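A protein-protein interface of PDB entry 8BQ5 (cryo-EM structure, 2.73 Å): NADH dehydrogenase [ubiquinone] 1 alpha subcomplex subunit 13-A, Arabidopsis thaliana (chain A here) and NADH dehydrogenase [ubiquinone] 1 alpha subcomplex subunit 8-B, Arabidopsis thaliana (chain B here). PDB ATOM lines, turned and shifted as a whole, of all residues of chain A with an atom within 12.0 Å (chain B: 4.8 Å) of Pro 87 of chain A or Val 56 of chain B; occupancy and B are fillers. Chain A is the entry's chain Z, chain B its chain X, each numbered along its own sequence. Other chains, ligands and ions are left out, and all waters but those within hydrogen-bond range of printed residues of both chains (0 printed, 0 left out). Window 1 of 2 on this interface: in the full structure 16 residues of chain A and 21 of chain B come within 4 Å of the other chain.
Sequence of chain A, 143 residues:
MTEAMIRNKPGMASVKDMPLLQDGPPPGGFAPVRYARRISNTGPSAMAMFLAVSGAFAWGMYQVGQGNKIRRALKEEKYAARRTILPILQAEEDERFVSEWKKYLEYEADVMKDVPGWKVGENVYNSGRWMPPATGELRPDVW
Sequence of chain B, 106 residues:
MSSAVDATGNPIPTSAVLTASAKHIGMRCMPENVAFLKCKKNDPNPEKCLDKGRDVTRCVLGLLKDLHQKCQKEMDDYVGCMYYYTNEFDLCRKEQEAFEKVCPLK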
ATOM      1  N   LYS A  78      -9.146  34.254 -16.161  1.00  0.00           N
ATOM      2  CA  LYS A  78      -9.969  33.112 -15.769  1.00  0.00           C
ATOM      3  C   LYS A  78      -9.729  31.916 -16.687  1.00  0.00           C
ATOM      4  O   LYS A  78      -9.555  30.779 -16.221  1.00  0.00           O
ATOM      5  CB  LYS A  78     -11.448  33.496 -15.769  1.00  0.00           C
ATOM      6  CG  LYS A  78     -12.363  32.377 -15.301  1.00  0.00           C
ATOM      7  CD  LYS A  78     -13.818  32.796 -15.316  1.00  0.00           C
ATOM      8  CE  LYS A  78     -14.322  33.001 -16.730  1.00  0.00           C
ATOM      9  NZ  LYS A  78     -14.320  31.724 -17.493  1.00  0.00           N
ATOM     10  N   TYR A  79      -9.686  32.162 -17.997  1.00  0.00           N
ATOM     11  CA  TYR A  79      -9.477  31.090 -18.963  1.00  0.00           C
ATOM     12  C   TYR A  79      -8.099  30.457 -18.808  1.00  0.00           C
ATOM     13  O   TYR A  79      -7.952  29.240 -18.965  1.00  0.00           O
ATOM     14  CB  TYR A  79      -9.665  31.628 -20.380  1.00  0.00           C
ATOM     15  CG  TYR A  79     -11.085  32.052 -20.678  1.00  0.00           C
ATOM     16  CD1 TYR A  79     -12.162  31.382 -20.115  1.00  0.00           C
ATOM     17  CD2 TYR A  79     -11.348  33.131 -21.512  1.00  0.00           C
ATOM     18  CE1 TYR A  79     -13.458  31.768 -20.379  1.00  0.00           C
ATOM     19  CE2 TYR A  79     -12.642  33.525 -21.780  1.00  0.00           C
ATOM     20  CZ  TYR A  79     -13.693  32.840 -21.212  1.00  0.00           C
ATOM     21  OH  TYR A  79     -14.987  33.225 -21.478  1.00  0.00           O
ATOM     22  N   ALA A  80      -7.080  31.267 -18.509  1.00  0.00           N
ATOM     23  CA  ALA A  80      -5.746  30.729 -18.270  1.00  0.00           C
ATOM     24  C   ALA A  80      -5.727  29.843 -17.034  1.00  0.00           C
ATOM     25  O   ALA A  80      -5.079  28.792 -17.026  1.00  0.00           O
ATOM     26  CB  ALA A  80      -4.738  31.868 -18.129  1.00  0.00           C
ATOM     27  N   ALA A  81      -6.428  30.254 -15.977  1.00  0.00           N
ATOM     28  CA  ALA A  81      -6.513  29.410 -14.790  1.00  0.00           C
ATOM     29  C   ALA A  81      -7.223  28.100 -15.097  1.00  0.00           C
ATOM     30  O   ALA A  81      -6.905  27.058 -14.512  1.00  0.00           O
ATOM     31  CB  ALA A  81      -7.229  30.150 -13.665  1.00  0.00           C
ATOM     32  N   ARG A  82      -8.199  28.132 -16.006  1.00  0.00           N
ATOM     33  CA  ARG A  82      -8.863  26.893 -16.396  1.00  0.00           C
ATOM     34  C   ARG A  82      -7.939  25.985 -17.199  1.00  0.00           C
ATOM     35  O   ARG A  82      -8.059  24.757 -17.124  1.00  0.00           O
ATOM     36  CB  ARG A  82     -10.123  27.205 -17.195  1.00  0.00           C
ATOM     37  CG  ARG A  82     -11.310  27.517 -16.318  1.00  0.00           C
ATOM     38  CD  ARG A  82     -12.461  28.071 -17.112  1.00  0.00           C
ATOM     39  NE  ARG A  82     -13.573  28.422 -16.239  1.00  0.00           N
ATOM     40  CZ  ARG A  82     -14.753  28.847 -16.665  1.00  0.00           C
ATOM     41  NH1 ARG A  82     -15.011  28.991 -17.954  1.00  0.00           N
ATOM     42  NH2 ARG A  82     -15.698  29.132 -15.775  1.00  0.00           N
ATOM     43  N   ARG A  83      -7.018  26.564 -17.969  1.00  0.00           N
ATOM     44  CA  ARG A  83      -6.178  25.758 -18.847  1.00  0.00           C
ATOM     45  C   ARG A  83      -5.059  25.051 -18.091  1.00  0.00           C
ATOM     46  O   ARG A  83      -4.610  23.982 -18.517  1.00  0.00           O
ATOM     47  CB  ARG A  83      -5.610  26.633 -19.963  1.00  0.00           C
ATOM     48  CG  ARG A  83      -6.521  26.713 -21.177  1.00  0.00           C
ATOM     49  CD  ARG A  83      -5.827  27.360 -22.355  1.00  0.00           C
ATOM     50  NE  ARG A  83      -5.508  28.754 -22.077  1.00  0.00           N
ATOM     51  CZ  ARG A  83      -6.276  29.780 -22.419  1.00  0.00           C
ATOM     52  NH1 ARG A  83      -7.408  29.604 -23.081  1.00  0.00           N
ATOM     53  NH2 ARG A  83      -5.897  31.011 -22.092  1.00  0.00           N
ATOM     54  N   THR A  84      -4.587  25.624 -16.982  1.00  0.00           N
ATOM     55  CA  THR A  84      -3.484  25.008 -16.251  1.00  0.00           C
ATOM     56  C   THR A  84      -3.930  23.820 -15.410  1.00  0.00           C
ATOM     57  O   THR A  84      -3.125  22.921 -15.144  1.00  0.00           O
ATOM     58  CB  THR A  84      -2.787  26.036 -15.360  1.00  0.00           C
ATOM     59  OG1 THR A  84      -3.646  26.393 -14.271  1.00  0.00           O
ATOM     60  CG2 THR A  84      -2.439  27.277 -16.157  1.00  0.00           C
ATOM     61  N   ILE A  85      -5.192  23.798 -14.974  1.00  0.00           N
ATOM     62  CA  ILE A  85      -5.702  22.708 -14.153  1.00  0.00           C
ATOM     63  C   ILE A  85      -6.540  21.724 -14.951  1.00  0.00           C
ATOM     64  O   ILE A  85      -7.072  20.767 -14.375  1.00  0.00           O
ATOM     65  CB  ILE A  85      -6.504  23.250 -12.954  1.00  0.00           C
ATOM     66  CG1 ILE A  85      -7.752  23.995 -13.428  1.00  0.00           C
ATOM     67  CG2 ILE A  85      -5.638  24.163 -12.110  1.00  0.00           C
ATOM     68  CD1 ILE A  85      -8.839  24.080 -12.380  1.00  0.00           C
ATOM     69  N   LEU A  86      -6.680  21.932 -16.259  1.00  0.00           N
ATOM     70  CA  LEU A  86      -7.405  20.973 -17.092  1.00  0.00           C
ATOM     71  C   LEU A  86      -6.777  19.585 -17.092  1.00  0.00           C
ATOM     72  O   LEU A  86      -7.530  18.600 -17.010  1.00  0.00           O
ATOM     73  CB  LEU A  86      -7.536  21.520 -18.519  1.00  0.00           C
ATOM     74  CG  LEU A  86      -8.388  20.736 -19.525  1.00  0.00           C
ATOM     75  CD1 LEU A  86      -9.039  21.684 -20.500  1.00  0.00           C
ATOM     76  CD2 LEU A  86      -7.571  19.708 -20.294  1.00  0.00           C
ATOM     77  N   PRO A  87      -5.453  19.418 -17.229  1.00  0.00           N
ATOM     78  CA  PRO A  87      -4.912  18.049 -17.329  1.00  0.00           C
ATOM     79  C   PRO A  87      -5.214  17.154 -16.138  1.00  0.00           C
ATOM     80  O   PRO A  87      -5.501  15.971 -16.341  1.00  0.00           O
ATOM     81  CB  PRO A  87      -3.408  18.287 -17.503  1.00  0.00           C
ATOM     82  CG  PRO A  87      -3.331  19.606 -18.161  1.00  0.00           C
ATOM     83  CD  PRO A  87      -4.408  20.419 -17.518  1.00  0.00           C
ATOM     84  N   ILE A  88      -5.176  17.665 -14.905  1.00  0.00           N
ATOM     85  CA  ILE A  88      -5.450  16.797 -13.760  1.00  0.00           C
ATOM     86  C   ILE A  88      -6.919  16.382 -13.739  1.00  0.00           C
ATOM     87  O   ILE A  88      -7.248  15.217 -13.470  1.00  0.00           O
ATOM     88  CB  ILE A  88      -5.020  17.471 -12.441  1.00  0.00           C
ATOM     89  CG1 ILE A  88      -5.293  16.534 -11.262  1.00  0.00           C
ATOM     90  CG2 ILE A  88      -5.697  18.819 -12.252  1.00  0.00           C
ATOM     91  CD1 ILE A  88      -5.106  17.168  -9.907  1.00  0.00           C
ATOM     92  N   LEU A  89      -7.821  17.319 -14.043  1.00  0.00           N
ATOM     93  CA  LEU A  89      -9.239  16.988 -14.132  1.00  0.00           C
ATOM     94  C   LEU A  89      -9.491  15.947 -15.214  1.00  0.00           C
ATOM     95  O   LEU A  89     -10.235  14.981 -15.003  1.00  0.00           O
ATOM     96  CB  LEU A  89     -10.049  18.253 -14.411  1.00  0.00           C
ATOM     97  CG  LEU A  89      -9.942  19.370 -13.373  1.00  0.00           C
ATOM     98  CD1 LEU A  89     -10.360  20.701 -13.975  1.00  0.00           C
ATOM     99  CD2 LEU A  89     -10.791  19.040 -12.166  1.00  0.00           C
ATOM    100  N   GLN A  90      -8.864  16.124 -16.379  1.00  0.00           N
ATOM    101  CA  GLN A  90      -9.031  15.174 -17.472  1.00  0.00           C
ATOM    102  C   GLN A  90      -8.475  13.806 -17.104  1.00  0.00           C
ATOM    103  O   GLN A  90      -9.066  12.781 -17.451  1.00  0.00           O
ATOM    104  CB  GLN A  90      -8.351  15.699 -18.735  1.00  0.00           C
ATOM    105  CG  GLN A  90      -8.924  15.143 -20.028  1.00  0.00           C
ATOM    106  CD  GLN A  90     -10.435  15.049 -20.007  1.00  0.00           C
ATOM    107  OE1 GLN A  90     -11.127  16.064 -19.978  1.00  0.00           O
ATOM    108  NE2 GLN A  90     -10.954  13.829 -20.037  1.00  0.00           N
ATOM    109  N   ALA A  91      -7.329  13.767 -16.421  1.00  0.00           N
ATOM    110  CA  ALA A  91      -6.747  12.492 -16.020  1.00  0.00           C
ATOM    111  C   ALA A  91      -7.660  11.752 -15.053  1.00  0.00           C
ATOM    112  O   ALA A  91      -7.874  10.538 -15.187  1.00  0.00           O
ATOM    113  CB  ALA A  91      -5.374  12.719 -15.393  1.00  0.00           C
ATOM    114  N   GLU A  92      -8.214  12.471 -14.076  1.00  0.00           N
ATOM    115  CA  GLU A  92      -9.147  11.850 -13.144  1.00  0.00           C
ATOM    116  C   GLU A  92     -10.382  11.332 -13.873  1.00  0.00           C
ATOM    117  O   GLU A  92     -10.856  10.219 -13.607  1.00  0.00           O
ATOM    118  CB  GLU A  92      -9.534  12.850 -12.059  1.00  0.00           C
ATOM    119  CG  GLU A  92     -10.811  12.508 -11.331  1.00  0.00           C
ATOM    120  CD  GLU A  92     -11.398  13.710 -10.633  1.00  0.00           C
ATOM    121  OE1 GLU A  92     -12.273  14.367 -11.232  1.00  0.00           O
ATOM    122  OE2 GLU A  92     -10.980  14.004  -9.494  1.00  0.00           O
ATOM    123  N   GLU A  93     -10.893  12.117 -14.820  1.00  0.00           N
ATOM    124  CA  GLU A  93     -12.095  11.694 -15.584  1.00  0.00           C
ATOM    125  C   GLU A  93     -11.758  10.455 -16.418  1.00  0.00           C
ATOM    126  O   GLU A  93     -12.612   9.557 -16.496  1.00  0.00           O
ATOM    127  CB  GLU A  93     -12.612  12.843 -16.454  1.00  0.00           C
ATOM    128  CG  GLU A  93     -13.715  12.439 -17.415  1.00  0.00           C
ATOM    129  CD  GLU A  93     -15.034  12.016 -16.789  1.00  0.00           C
ATOM    130  OE1 GLU A  93     -15.720  11.167 -17.390  1.00  0.00           O
ATOM    131  OE2 GLU A  93     -15.379  12.541 -15.712  1.00  0.00           O
ATOM    132  N   ASP A  94     -10.566  10.412 -17.008  1.00  0.00           N
ATOM    133  CA  ASP A  94     -10.168   9.257 -17.805  1.00  0.00           C
ATOM    134  C   ASP A  94     -10.094   8.003 -16.947  1.00  0.00           C
ATOM    135  O   ASP A  94     -10.579   6.937 -17.343  1.00  0.00           O
ATOM    136  CB  ASP A  94      -8.819   9.518 -18.477  1.00  0.00           C
ATOM    137  CG  ASP A  94      -8.922  10.468 -19.653  1.00  0.00           C
ATOM    138  OD1 ASP A  94     -10.034  10.958 -19.934  1.00  0.00           O
ATOM    139  OD2 ASP A  94      -7.886  10.710 -20.307  1.00  0.00           O
ATOM    140  N   GLU A  95      -9.484   8.114 -15.764  1.00  0.00           N
ATOM    141  CA  GLU A  95      -9.397   6.959 -14.873  1.00  0.00           C
ATOM    142  C   GLU A  95     -10.779   6.485 -14.442  1.00  0.00           C
ATOM    143  O   GLU A  95     -11.065   5.276 -14.446  1.00  0.00           O
ATOM    144  CB  GLU A  95      -8.542   7.300 -13.652  1.00  0.00           C
ATOM    145  CG  GLU A  95      -7.163   6.655 -13.650  1.00  0.00           C
ATOM    146  CD  GLU A  95      -7.194   5.174 -14.003  1.00  0.00           C
ATOM    147  OE1 GLU A  95      -8.168   4.483 -13.635  1.00  0.00           O
ATOM    148  OE2 GLU A  95      -6.237   4.699 -14.649  1.00  0.00           O
ATOM    149  N   ARG A  96     -11.640   7.426 -14.063  1.00  0.00           N
ATOM    150  CA  ARG A  96     -13.027   7.085 -13.653  1.00  0.00           C
ATOM    151  C   ARG A  96     -13.746   6.377 -14.805  1.00  0.00           C
ATOM    152  O   ARG A  96     -14.398   5.363 -14.544  1.00  0.00           O
ATOM    153  CB  ARG A  96     -13.742   8.362 -13.200  1.00  0.00           C
ATOM    154  CG  ARG A  96     -15.183   8.181 -12.755  1.00  0.00           C
ATOM    155  CD  ARG A  96     -16.009   9.354 -13.245  1.00  0.00           C
ATOM    156  NE  ARG A  96     -16.197   9.301 -14.689  1.00  0.00           N
ATOM    157  CZ  ARG A  96     -17.164   8.625 -15.295  1.00  0.00           C
ATOM    158  NH1 ARG A  96     -18.045   7.946 -14.582  1.00  0.00           N
ATOM    159  NH2 ARG A  96     -17.250   8.633 -16.613  1.00  0.00           N
ATOM    160  N   GLU B  32       4.605  18.388 -17.803  1.00  0.00           N
ATOM    161  CA  GLU B  32       3.664  17.243 -17.701  1.00  0.00           C
ATOM    162  C   GLU B  32       2.346  17.646 -18.365  1.00  0.00           C
ATOM    163  O   GLU B  32       1.792  16.822 -19.117  1.00  0.00           O
ATOM    164  CB  GLU B  32       3.481  16.817 -16.243  1.00  0.00           C
ATOM    165  CG  GLU B  32       4.648  16.023 -15.690  1.00  0.00           C
ATOM    166  CD  GLU B  32       5.870  16.859 -15.353  1.00  0.00           C
ATOM    167  OE1 GLU B  32       6.980  16.468 -15.764  1.00  0.00           O
ATOM    168  OE2 GLU B  32       5.707  17.894 -14.680  1.00  0.00           O
ATOM    169  N   ASN B  33       1.887  18.873 -18.126  1.00  0.00           N
ATOM    170  CA  ASN B  33       0.639  19.378 -18.755  1.00  0.00           C
ATOM    171  C   ASN B  33       0.756  19.284 -20.278  1.00  0.00           C
ATOM    172  O   ASN B  33      -0.172  18.745 -20.885  1.00  0.00           O
ATOM    173  CB  ASN B  33       0.341  20.804 -18.293  1.00  0.00           C
ATOM    174  CG  ASN B  33      -0.193  20.891 -16.879  1.00  0.00           C
ATOM    175  OD1 ASN B  33      -0.374  19.878 -16.210  1.00  0.00           O
ATOM    176  ND2 ASN B  33      -0.444  22.103 -16.415  1.00  0.00           N
ATOM    177  N   PHE B  36       0.738  15.594 -21.558  1.00  0.00           N
ATOM    178  CA  PHE B  36      -0.606  15.037 -21.475  1.00  0.00           C
ATOM    179  C   PHE B  36      -1.491  15.578 -22.589  1.00  0.00           C
ATOM    180  O   PHE B  36      -2.243  14.823 -23.219  1.00  0.00           O
ATOM    181  CB  PHE B  36      -1.205  15.349 -20.104  1.00  0.00           C
ATOM    182  CG  PHE B  36      -2.599  14.828 -19.914  1.00  0.00           C
ATOM    183  CD1 PHE B  36      -2.816  13.511 -19.552  1.00  0.00           C
ATOM    184  CD2 PHE B  36      -3.693  15.660 -20.087  1.00  0.00           C
ATOM    185  CE1 PHE B  36      -4.097  13.031 -19.373  1.00  0.00           C
ATOM    186  CE2 PHE B  36      -4.975  15.186 -19.912  1.00  0.00           C
ATOM    187  CZ  PHE B  36      -5.178  13.870 -19.554  1.00  0.00           C
ATOM    188  N   LEU B  37      -1.410  16.884 -22.853  1.00  0.00           N
ATOM    189  CA  LEU B  37      -2.242  17.479 -23.893  1.00  0.00           C
ATOM    190  C   LEU B  37      -1.845  16.984 -25.278  1.00  0.00           C
ATOM    191  O   LEU B  37      -2.710  16.770 -26.132  1.00  0.00           O
ATOM    192  CB  LEU B  37      -2.165  19.001 -23.812  1.00  0.00           C
ATOM    193  CG  LEU B  37      -2.806  19.561 -22.545  1.00  0.00           C
ATOM    194  CD1 LEU B  37      -2.615  21.062 -22.448  1.00  0.00           C
ATOM    195  CD2 LEU B  37      -4.278  19.189 -22.500  1.00  0.00           C
ATOM    196  N   LYS B  52       0.651   9.364 -18.746  1.00  0.00           N
ATOM    197  CA  LYS B  52       0.800  10.815 -18.682  1.00  0.00           C
ATOM    198  C   LYS B  52      -0.142  11.414 -17.646  1.00  0.00           C
ATOM    199  O   LYS B  52       0.209  12.382 -16.961  1.00  0.00           O
ATOM    200  CB  LYS B  52       0.557  11.433 -20.057  1.00  0.00           C
ATOM    201  CG  LYS B  52       1.615  11.068 -21.081  1.00  0.00           C
ATOM    202  CD  LYS B  52       1.309  11.688 -22.432  1.00  0.00           C
ATOM    203  CE  LYS B  52       2.382  11.341 -23.451  1.00  0.00           C
ATOM    204  NZ  LYS B  52       2.093  11.918 -24.792  1.00  0.00           N
ATOM    205  N   GLY B  53      -1.343  10.849 -17.518  1.00  0.00           N
ATOM    206  CA  GLY B  53      -2.258  11.310 -16.488  1.00  0.00           C
ATOM    207  C   GLY B  53      -1.718  11.093 -15.088  1.00  0.00           C
ATOM    208  O   GLY B  53      -1.862  11.953 -14.217  1.00  0.00           O
ATOM    209  N   ARG B  54      -1.092   9.936 -14.850  1.00  0.00           N
ATOM    210  CA  ARG B  54      -0.463   9.694 -13.555  1.00  0.00           C
ATOM    211  C   ARG B  54       0.671  10.677 -13.305  1.00  0.00           C
ATOM    212  O   ARG B  54       0.836  11.170 -12.185  1.00  0.00           O
ATOM    213  CB  ARG B  54       0.055   8.258 -13.469  1.00  0.00           C
ATOM    214  CG  ARG B  54      -1.025   7.197 -13.464  1.00  0.00           C
ATOM    215  CD  ARG B  54      -0.427   5.824 -13.220  1.00  0.00           C
ATOM    216  NE  ARG B  54      -0.166   5.104 -14.459  1.00  0.00           N
ATOM    217  CZ  ARG B  54      -1.045   4.320 -15.066  1.00  0.00           C
ATOM    218  NH1 ARG B  54      -2.261   4.139 -14.580  1.00  0.00           N
ATOM    219  NH2 ARG B  54      -0.694   3.702 -16.191  1.00  0.00           N
ATOM    220  N   ASP B  55       1.466  10.968 -14.336  1.00  0.00           N
ATOM    221  CA  ASP B  55       2.529  11.961 -14.198  1.00  0.00           C
ATOM    222  C   ASP B  55       1.960  13.315 -13.785  1.00  0.00           C
ATOM    223  O   ASP B  55       2.462  13.965 -12.853  1.00  0.00           O
ATOM    224  CB  ASP B  55       3.294  12.088 -15.515  1.00  0.00           C
ATOM    225  CG  ASP B  55       4.582  11.297 -15.524  1.00  0.00           C
ATOM    226  OD1 ASP B  55       5.327  11.397 -16.520  1.00  0.00           O
ATOM    227  OD2 ASP B  55       4.847  10.575 -14.541  1.00  0.00           O
ATOM    228  N   VAL B  56       0.911  13.755 -14.481  1.00  0.00           N
ATOM    229  CA  VAL B  56       0.295  15.050 -14.200  1.00  0.00           C
ATOM    230  C   VAL B  56      -0.258  15.077 -12.780  1.00  0.00           C
ATOM    231  O   VAL B  56      -0.057  16.044 -12.032  1.00  0.00           O
ATOM    232  CB  VAL B  56      -0.802  15.351 -15.239  1.00  0.00           C
ATOM    233  CG1 VAL B  56      -1.837  16.306 -14.671  1.00  0.00           C
ATOM    234  CG2 VAL B  56      -0.193  15.911 -16.508  1.00  0.00           C
ATOM    235  N   THR B  57      -0.968  14.015 -12.392  1.00  0.00           N
ATOM    236  CA  THR B  57      -1.556  13.956 -11.061  1.00  0.00           C
ATOM    237  C   THR B  57      -0.479  13.984  -9.986  1.00  0.00           C
ATOM    238  O   THR B  57      -0.627  14.664  -8.965  1.00  0.00           O
ATOM    239  CB  THR B  57      -2.414  12.698 -10.923  1.00  0.00           C
ATOM    240  OG1 THR B  57      -3.327  12.615 -12.025  1.00  0.00           O
ATOM    241  CG2 THR B  57      -3.197  12.727  -9.623  1.00  0.00           C
ATOM    242  N   ARG B  58       0.618  13.256 -10.204  1.00  0.00           N
ATOM    243  CA  ARG B  58       1.712  13.240  -9.239  1.00  0.00           C
ATOM    244  C   ARG B  58       2.368  14.621  -9.066  1.00  0.00           C
ATOM    245  O   ARG B  58       2.525  15.076  -7.931  1.00  0.00           O
ATOM    246  CB  ARG B  58       2.756  12.210  -9.673  1.00  0.00           C
ATOM    247  CG  ARG B  58       4.043  12.229  -8.874  1.00  0.00           C
ATOM    248  CD  ARG B  58       4.964  11.075  -9.267  1.00  0.00           C
ATOM    249  NE  ARG B  58       4.925  10.777 -10.695  1.00  0.00           N
ATOM    250  CZ  ARG B  58       4.402   9.676 -11.219  1.00  0.00           C
ATOM    251  NH1 ARG B  58       3.859   8.739 -10.458  1.00  0.00           N
ATOM    252  NH2 ARG B  58       4.425   9.510 -12.538  1.00  0.00           N
ATOM    253  N   CYS B  59       2.673  15.323 -10.162  1.00  0.00           N
ATOM    254  CA  CYS B  59       3.252  16.693 -10.071  1.00  0.00           C
ATOM    255  C   CYS B  59       2.291  17.626  -9.331  1.00  0.00           C
ATOM    256  O   CYS B  59       2.768  18.378  -8.468  1.00  0.00           O
ATOM    257  CB  CYS B  59       3.523  17.292 -11.446  1.00  0.00           C
ATOM    258  SG  CYS B  59       4.310  18.923 -11.372  1.00  0.00           S
ATOM    259  N   VAL B  60       1.000  17.599  -9.677  1.00  0.00           N
ATOM    260  CA  VAL B  60       0.034  18.552  -9.055  1.00  0.00           C
ATOM    261  C   VAL B  60      -0.073  18.221  -7.560  1.00  0.00           C
ATOM    262  O   VAL B  60       0.051  19.152  -6.757  1.00  0.00           O
ATOM    263  CB  VAL B  60      -1.342  18.555  -9.754  1.00  0.00           C
ATOM    264  CG1 VAL B  60      -2.348  19.416  -9.008  1.00  0.00           C
ATOM    265  CG2 VAL B  60      -1.235  19.005 -11.202  1.00  0.00           C
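Among the printed residues, merely in contact across the chains: Pro 87 of chain A with Asn 33 of chain B, Ala 91 of chain A with Gly 53 of chain B, Gln 90 of chain A with Phe 36 of chain B, Ile 88 of chain A with Val 56 of chain B, Ile 88 of chain A with Val 60 of chain B, Pro 87 of chain A with Phe 36 of chain B, Pro 87 of chain A with Val 56 of chain B, Ala 91 of chain A with Phe 36 of chain B, Ala 91 of chain A with Thr 57 of chain B and Leu 86 of chain A with Leu 37 of chain B.
The backbone carbonyl oxygen of Gly 53 of chain B sits at hydrogen-bond distance from the side-chain hydroxyl of Thr 57 of chain B (2.7 Å). The side-chain amide nitrogen (NE2) of Gln 90 of chain A is in hydrogen-bond range of the side-chain carboxylate (OD1) of Asp 94 of chain A, 3.0 Å away. The backbone carbonyl oxygen (O) of Ala 81 of chain A is in hydrogen-bond range of the side-chain hydroxyl (OG1) of Thr 84 of chain A (3.3 Å).
Pro 87 of chain A touches just these residues of chain B: Asn 33, Phe 36 and Val 56. Val 56 of chain B touches just these residues of chain A: Pro 87 and Ile 88. Glu 32 of chain B touches none of the printed residues of chain A. Asp 55 of chain B touches none of the printed residues of chain A. No residue of chain A comes within 4 Å of Cys 59 of chain B. Of chain A, only Ile 88 comes within 4 Å of Val 60 of chain B. Of the printed residues of chain B, Leu 86 of chain A touches Leu 37 (3.997 Å). Printed residues of chain B within 4 Å of Gln 90 of chain A: Phe 36 (3.6 Å). Of the printed residues of chain B, Ile 88 of chain A touches Val 56 (3.6 Å) and Val 60 (3.7 Å). Printed residues of chain B within 4 Å of Thr 84 of chain A: Asn 33. Printed residues of chain B within 4 Å of Ala 91 of chain A: Phe 36 (3.8 Å), Gly 53 (3.6 Å) and Thr 57 (3.9 Å). Arg 54 of chain B touches none of the printed residues of chain A. Ala 80 of chain A touches none of the printed residues of chain B. The nearest residue of chain A that does not touch Val 56 of chain B is Ala 91 of chain A (5.1 Å).
The backbone carbonyl oxygen of Thr 84 of chain A is in hydrogen-bond range of the side-chain amide nitrogen of Asn 33 of chain B, 3.1 Å away.
Printed residues of chain A that touch a printed residue of chain B: Thr 84, Leu 86, Pro 87, Ile 88, Gln 90 and Ala 91. Along chain B the printed residues that touch a printed residue of chain A span positions 33 to 60.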
